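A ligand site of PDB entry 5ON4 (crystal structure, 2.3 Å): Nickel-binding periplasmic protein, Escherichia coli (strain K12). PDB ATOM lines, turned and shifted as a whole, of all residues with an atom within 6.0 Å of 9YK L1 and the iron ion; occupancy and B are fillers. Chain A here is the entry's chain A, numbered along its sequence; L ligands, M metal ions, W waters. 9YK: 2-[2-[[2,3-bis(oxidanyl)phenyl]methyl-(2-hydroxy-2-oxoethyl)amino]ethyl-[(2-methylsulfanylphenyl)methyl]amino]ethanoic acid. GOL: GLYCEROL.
The guanidinium group of Arg 137 is in salt-bridge range of an oxygen (OXT) of 9YK L1 (2.4 Å). An oxygen (OBD) of 9YK L1 lies within hydrogen-bond range of a ring nitrogen (NE2) of His 416 (3.1 Å).
The side-chain hydroxyl (OH) of Tyr 22 sits at hydrogen-bond distance from the indole nitrogen (NE1) of Trp 100 (2.7 Å). The side-chain sulfur (SD) of Met 27 sits close to the side-chain hydroxyl (OG1) of Thr 490 (3.6 Å).
The side-chain sulfur (SD) of Met 27 lies close to an oxygen (OXT) of 9YK L1, 3.8 Å away. Residues that only touch 9YK L1: Tyr 22, Trp 398, Thr 23, Trp 100 and Tyr 402. Within 4 Å of 9YK L1: Tyr 22, Thr 23, Met 27, Trp 100, Arg 137, Trp 398, Tyr 402 and His 416.
No residue comes within 4 Å of the iron ion. The nearest printed residue that does not touch the iron ion is Arg 137 (4.5 Å).
The iron ion is bound by an oxygen (OAY) of 9YK L1 (2.0 Å), an oxygen (O3) of GOL L2 (2.2 Å), an oxygen (O) of 9YK L1 (2.2 Å), a nitrogen (N) of 9YK L1 (2.3 Å) and a nitrogen (NAL) of 9YK L1 (2.4 Å). Slightly farther from the iron ion lies SBB of 9YK L1 (3.0 Å).
Water W1 lies within hydrogen-bond range of the side-chain hydroxyl of Tyr 402 (2.9 Å), an oxygen (OXT) of 9YK L1 (3.0 Å) and the backbone carbonyl oxygen of Arg 137 (3.2 Å).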
ATOM      1  N   TYR A  22       1.374  11.588  10.921  1.00  0.00           N
ATOM      2  CA  TYR A  22       2.692  11.354  11.495  1.00  0.00           C
ATOM      3  C   TYR A  22       3.777  11.984  10.631  1.00  0.00           C
ATOM      4  O   TYR A  22       3.603  13.099  10.139  1.00  0.00           O
ATOM      5  CB  TYR A  22       2.916   9.858  11.683  1.00  0.00           C
ATOM      6  CG  TYR A  22       1.849   9.235  12.552  1.00  0.00           C
ATOM      7  CD1 TYR A  22       1.933   9.291  13.941  1.00  0.00           C
ATOM      8  CD2 TYR A  22       0.743   8.611  11.995  1.00  0.00           C
ATOM      9  CE1 TYR A  22       0.960   8.733  14.741  1.00  0.00           C
ATOM     10  CE2 TYR A  22      -0.238   8.050  12.792  1.00  0.00           C
ATOM     11  CZ  TYR A  22      -0.131   8.119  14.159  1.00  0.00           C
ATOM     12  OH  TYR A  22      -1.108   7.553  14.948  1.00  0.00           O
ATOM     13  N   THR A  23       4.891  11.282  10.439  1.00  0.00           N
ATOM     14  CA  THR A  23       5.987  11.795   9.618  1.00  0.00           C
ATOM     15  C   THR A  23       5.450  12.179   8.233  1.00  0.00           C
ATOM     16  O   THR A  23       4.592  11.482   7.689  1.00  0.00           O
ATOM     17  CB  THR A  23       7.146  10.753   9.502  1.00  0.00           C
ATOM     18  OG1 THR A  23       8.302  11.384   8.926  1.00  0.00           O
ATOM     19  CG2 THR A  23       6.740   9.553   8.666  1.00  0.00           C
ATOM     20  N   MET A  27       6.695  16.056  15.985  1.00  0.00           N
ATOM     21  CA  MET A  27       5.861  16.010  17.184  1.00  0.00           C
ATOM     22  C   MET A  27       6.030  17.241  18.066  1.00  0.00           C
ATOM     23  O   MET A  27       5.044  17.732  18.636  1.00  0.00           O
ATOM     24  CB  MET A  27       6.164  14.754  17.996  1.00  0.00           C
ATOM     25  CG  MET A  27       6.139  13.468  17.190  1.00  0.00           C
ATOM     26  SD  MET A  27       6.260  11.989  18.203  1.00  0.00           S
ATOM     27  CE  MET A  27       4.727  12.081  19.127  1.00  0.00           C
ATOM     28  N   ARG A  97      -4.593   3.457  10.152  1.00  0.00           N
ATOM     29  CA  ARG A  97      -3.235   3.972  10.301  1.00  0.00           C
ATOM     30  C   ARG A  97      -2.847   4.135  11.761  1.00  0.00           C
ATOM     31  O   ARG A  97      -1.661   4.155  12.099  1.00  0.00           O
ATOM     32  CB  ARG A  97      -3.104   5.326   9.586  1.00  0.00           C
ATOM     33  CG  ARG A  97      -1.675   5.637   9.158  1.00  0.00           C
ATOM     34  CD  ARG A  97      -1.626   6.171   7.735  1.00  0.00           C
ATOM     35  NE  ARG A  97      -0.270   6.550   7.315  1.00  0.00           N
ATOM     36  CZ  ARG A  97       0.458   7.535   7.837  1.00  0.00           C
ATOM     37  NH1 ARG A  97      -0.016   8.287   8.821  1.00  0.00           N
ATOM     38  NH2 ARG A  97       1.672   7.774   7.364  1.00  0.00           N
ATOM     39  N   TRP A 100      -1.413   1.179  15.836  1.00  0.00           N
ATOM     40  CA  TRP A 100      -0.389   1.069  16.865  1.00  0.00           C
ATOM     41  C   TRP A 100      -0.923   1.570  18.202  1.00  0.00           C
ATOM     42  O   TRP A 100      -0.615   0.998  19.254  1.00  0.00           O
ATOM     43  CB  TRP A 100       0.861   1.864  16.470  1.00  0.00           C
ATOM     44  CG  TRP A 100       0.683   3.343  16.567  1.00  0.00           C
ATOM     45  CD1 TRP A 100       0.175   4.179  15.613  1.00  0.00           C
ATOM     46  CD2 TRP A 100       0.981   4.177  17.699  1.00  0.00           C
ATOM     47  NE1 TRP A 100       0.154   5.467  16.078  1.00  0.00           N
ATOM     48  CE2 TRP A 100       0.639   5.495  17.351  1.00  0.00           C
ATOM     49  CE3 TRP A 100       1.511   3.922  18.970  1.00  0.00           C
ATOM     50  CZ2 TRP A 100       0.805   6.570  18.227  1.00  0.00           C
ATOM     51  CZ3 TRP A 100       1.681   4.991  19.839  1.00  0.00           C
ATOM     52  CH2 TRP A 100       1.333   6.296  19.457  1.00  0.00           C
ATOM     53  N   ARG A 137       0.000  13.551  19.394  1.00  0.00           N
ATOM     54  CA  ARG A 137      -0.818  13.209  18.235  1.00  0.00           C
ATOM     55  C   ARG A 137      -1.384  11.811  18.438  1.00  0.00           C
ATOM     56  O   ARG A 137      -0.832  11.025  19.213  1.00  0.00           O
ATOM     57  CB  ARG A 137       0.013  13.295  16.955  1.00  0.00           C
ATOM     58  CG  ARG A 137       1.204  12.360  16.890  1.00  0.00           C
ATOM     59  CD  ARG A 137       2.207  12.846  15.853  1.00  0.00           C
ATOM     60  NE  ARG A 137       3.281  11.893  15.605  1.00  0.00           N
ATOM     61  CZ  ARG A 137       4.288  12.105  14.773  1.00  0.00           C
ATOM     62  NH1 ARG A 137       4.373  13.253  14.113  1.00  0.00           N
ATOM     63  NH2 ARG A 137       5.222  11.188  14.608  1.00  0.00           N
ATOM     64  N   GLN A 385      12.777  -3.426   9.675  1.00  0.00           N
ATOM     65  CA  GLN A 385      12.022  -3.504  10.913  1.00  0.00           C
ATOM     66  C   GLN A 385      10.594  -3.980  10.647  1.00  0.00           C
ATOM     67  O   GLN A 385      10.094  -4.849  11.357  1.00  0.00           O
ATOM     68  CB  GLN A 385      12.001  -2.139  11.616  1.00  0.00           C
ATOM     69  CG  GLN A 385      13.230  -1.871  12.460  1.00  0.00           C
ATOM     70  CD  GLN A 385      13.163  -0.553  13.195  1.00  0.00           C
ATOM     71  OE1 GLN A 385      12.361   0.315  12.859  1.00  0.00           O
ATOM     72  NE2 GLN A 385      14.005  -0.391  14.209  1.00  0.00           N
ATOM     73  N   HIS A 395      17.134  -0.304  18.971  1.00  0.00           N
ATOM     74  CA  HIS A 395      15.750   0.043  19.272  1.00  0.00           C
ATOM     75  C   HIS A 395      15.656   0.952  20.495  1.00  0.00           C
ATOM     76  O   HIS A 395      16.572   1.025  21.305  1.00  0.00           O
ATOM     77  CB  HIS A 395      14.924  -1.235  19.478  1.00  0.00           C
ATOM     78  CG  HIS A 395      13.469  -1.069  19.200  1.00  0.00           C
ATOM     79  ND1 HIS A 395      12.969  -0.042  18.415  1.00  0.00           N
ATOM     80  CD2 HIS A 395      12.387  -1.784  19.595  1.00  0.00           C
ATOM     81  CE1 HIS A 395      11.656  -0.136  18.346  1.00  0.00           C
ATOM     82  NE2 HIS A 395      11.277  -1.192  19.047  1.00  0.00           N
ATOM     83  N   ARG A 396      14.521   1.634  20.596  1.00  0.00           N
ATOM     84  CA  ARG A 396      14.291   2.632  21.633  1.00  0.00           C
ATOM     85  C   ARG A 396      12.921   2.431  22.245  1.00  0.00           C
ATOM     86  O   ARG A 396      11.969   2.096  21.532  1.00  0.00           O
ATOM     87  CB  ARG A 396      14.386   4.039  21.047  1.00  0.00           C
ATOM     88  CG  ARG A 396      15.584   4.868  21.469  1.00  0.00           C
ATOM     89  CD  ARG A 396      15.602   6.179  20.706  1.00  0.00           C
ATOM     90  NE  ARG A 396      16.902   6.836  20.705  1.00  0.00           N
ATOM     91  CZ  ARG A 396      17.758   6.814  19.679  1.00  0.00           C
ATOM     92  NH1 ARG A 396      17.442   6.147  18.574  1.00  0.00           N
ATOM     93  NH2 ARG A 396      18.912   7.444  19.760  1.00  0.00           N
ATOM     94  N   TRP A 398       9.899   4.629  24.383  1.00  0.00           N
ATOM     95  CA  TRP A 398       9.329   5.904  23.963  1.00  0.00           C
ATOM     96  C   TRP A 398       9.223   6.922  25.081  1.00  0.00           C
ATOM     97  O   TRP A 398       8.860   8.077  24.840  1.00  0.00           O
ATOM     98  CB  TRP A 398       7.958   5.662  23.339  1.00  0.00           C
ATOM     99  CG  TRP A 398       8.016   4.876  22.070  1.00  0.00           C
ATOM    100  CD1 TRP A 398       9.093   4.738  21.242  1.00  0.00           C
ATOM    101  CD2 TRP A 398       6.951   4.119  21.477  1.00  0.00           C
ATOM    102  NE1 TRP A 398       8.773   3.939  20.180  1.00  0.00           N
ATOM    103  CE2 TRP A 398       7.454   3.553  20.296  1.00  0.00           C
ATOM    104  CE3 TRP A 398       5.626   3.878  21.838  1.00  0.00           C
ATOM    105  CZ2 TRP A 398       6.689   2.748  19.467  1.00  0.00           C
ATOM    106  CZ3 TRP A 398       4.859   3.081  21.003  1.00  0.00           C
ATOM    107  CH2 TRP A 398       5.390   2.517  19.835  1.00  0.00           C
ATOM    108  N   TYR A 402       4.308   6.995  27.151  1.00  0.00           N
ATOM    109  CA  TYR A 402       4.140   5.794  26.342  1.00  0.00           C
ATOM    110  C   TYR A 402       4.580   4.530  27.077  1.00  0.00           C
ATOM    111  O   TYR A 402       4.067   3.447  26.829  1.00  0.00           O
ATOM    112  CB  TYR A 402       4.911   5.912  25.035  1.00  0.00           C
ATOM    113  CG  TYR A 402       4.555   7.104  24.183  1.00  0.00           C
ATOM    114  CD1 TYR A 402       5.142   8.352  24.417  1.00  0.00           C
ATOM    115  CD2 TYR A 402       3.642   6.999  23.145  1.00  0.00           C
ATOM    116  CE1 TYR A 402       4.822   9.448  23.647  1.00  0.00           C
ATOM    117  CE2 TYR A 402       3.312   8.099  22.367  1.00  0.00           C
ATOM    118  CZ  TYR A 402       3.908   9.311  22.617  1.00  0.00           C
ATOM    119  OH  TYR A 402       3.589  10.407  21.847  1.00  0.00           O
ATOM    120  N   SER A 415       3.458  -4.463  11.805  1.00  0.00           N
ATOM    121  CA  SER A 415       4.297  -3.481  11.116  1.00  0.00           C
ATOM    122  C   SER A 415       5.472  -3.007  11.980  1.00  0.00           C
ATOM    123  O   SER A 415       6.387  -2.359  11.484  1.00  0.00           O
ATOM    124  CB  SER A 415       3.439  -2.269  10.697  1.00  0.00           C
ATOM    125  OG  SER A 415       4.214  -1.274  10.057  1.00  0.00           O
ATOM    126  N   HIS A 416       5.438  -3.338  13.266  1.00  0.00           N
ATOM    127  CA  HIS A 416       6.427  -2.847  14.213  1.00  0.00           C
ATOM    128  C   HIS A 416       7.530  -3.864  14.481  1.00  0.00           C
ATOM    129  O   HIS A 416       7.284  -5.069  14.512  1.00  0.00           O
ATOM    130  CB  HIS A 416       5.750  -2.443  15.522  1.00  0.00           C
ATOM    131  CG  HIS A 416       6.465  -1.361  16.262  1.00  0.00           C
ATOM    132  ND1 HIS A 416       6.473  -1.275  17.641  1.00  0.00           N
ATOM    133  CD2 HIS A 416       7.206  -0.313  15.818  1.00  0.00           C
ATOM    134  CE1 HIS A 416       7.175  -0.228  18.017  1.00  0.00           C
ATOM    135  NE2 HIS A 416       7.633   0.378  16.930  1.00  0.00           N
ATOM    136  N   THR A 490       9.168  13.898  23.617  1.00  0.00           N
ATOM    137  CA  THR A 490       9.215  14.446  22.263  1.00  0.00           C
ATOM    138  C   THR A 490       8.828  15.915  22.212  1.00  0.00           C
ATOM    139  O   THR A 490       8.915  16.557  21.160  1.00  0.00           O
ATOM    140  CB  THR A 490       8.301  13.653  21.317  1.00  0.00           C
ATOM    141  OG1 THR A 490       8.474  14.122  19.979  1.00  0.00           O
ATOM    142  CG2 THR A 490       6.845  13.823  21.720  1.00  0.00           C
HETATM  143  CAR 9YK L   1       8.912   8.829  18.813  1.00  0.00           C
HETATM  144  CAS 9YK L   1       8.003   7.904  18.296  1.00  0.00           C
HETATM  145  OAY 9YK L   1       8.114   7.497  16.981  1.00  0.00           O
HETATM  146  CAQ 9YK L   1       8.808   9.248  20.125  1.00  0.00           C
HETATM  147  CAE 9YK L   1       7.801   8.743  20.936  1.00  0.00           C
HETATM  148  CAF 9YK L   1       6.888   7.816  20.433  1.00  0.00           C
HETATM  149  CAG 9YK L   1       6.978   7.385  19.108  1.00  0.00           C
HETATM  150  CAH 9YK L   1       5.980   6.384  18.579  1.00  0.00           C
HETATM  151  N   9YK L   1       5.264   6.941  17.417  1.00  0.00           N
HETATM  152  CA  9YK L   1       4.426   8.062  17.817  1.00  0.00           C
HETATM  153  C   9YK L   1       4.410   9.075  16.730  1.00  0.00           C
HETATM  154  OXT 9YK L   1       3.435   9.864  16.902  1.00  0.00           O
HETATM  155  O   9YK L   1       5.358   8.868  15.941  1.00  0.00           O
HETATM  156  CAJ 9YK L   1       4.417   5.926  16.731  1.00  0.00           C
HETATM  157  CAK 9YK L   1       5.136   4.589  16.577  1.00  0.00           C
HETATM  158  NAL 9YK L   1       6.380   4.714  15.775  1.00  0.00           N
HETATM  159  CAT 9YK L   1       7.239   3.548  15.901  1.00  0.00           C
HETATM  160  CAZ 9YK L   1       8.570   3.963  16.429  1.00  0.00           C
HETATM  161  OBD 9YK L   1       9.306   2.954  16.609  1.00  0.00           O
HETATM  162  OBA 9YK L   1       8.632   5.217  16.541  1.00  0.00           O
HETATM  163  CAM 9YK L   1       6.262   5.127  14.364  1.00  0.00           C
HETATM  164  CAN 9YK L   1       4.928   4.920  13.608  1.00  0.00           C
HETATM  165  CAO 9YK L   1       4.304   3.673  13.537  1.00  0.00           C
HETATM  166  CAP 9YK L   1       3.092   3.533  12.843  1.00  0.00           C
HETATM  167  CAW 9YK L   1       2.524   4.629  12.200  1.00  0.00           C
HETATM  168  CAV 9YK L   1       3.145   5.870  12.247  1.00  0.00           C
HETATM  169  CAU 9YK L   1       4.354   6.015  12.949  1.00  0.00           C
HETATM  170  SBB 9YK L   1       5.148   7.592  13.017  1.00  0.00           S
HETATM  171  CBE 9YK L   1       6.445   7.661  11.807  1.00  0.00           C
HETATM  172  C1  GOL L   2      10.230   7.617  13.706  1.00  0.00           C
HETATM  173  O1  GOL L   2      10.958   6.960  14.730  1.00  0.00           O
HETATM  174  C2  GOL L   2      10.103   9.103  14.037  1.00  0.00           C
HETATM  175  O2  GOL L   2      10.693   9.366  15.280  1.00  0.00           O
HETATM  176  C3  GOL L   2       8.640   9.504  14.076  1.00  0.00           C
HETATM  177  O3  GOL L   2       7.945   8.707  15.013  1.00  0.00           O
HETATM  178 FE    FE M   1       6.657   7.091  15.617  1.00  0.00          FE
HETATM  179  O   HOH W   1       2.022   9.713  19.533  1.00  0.00           O
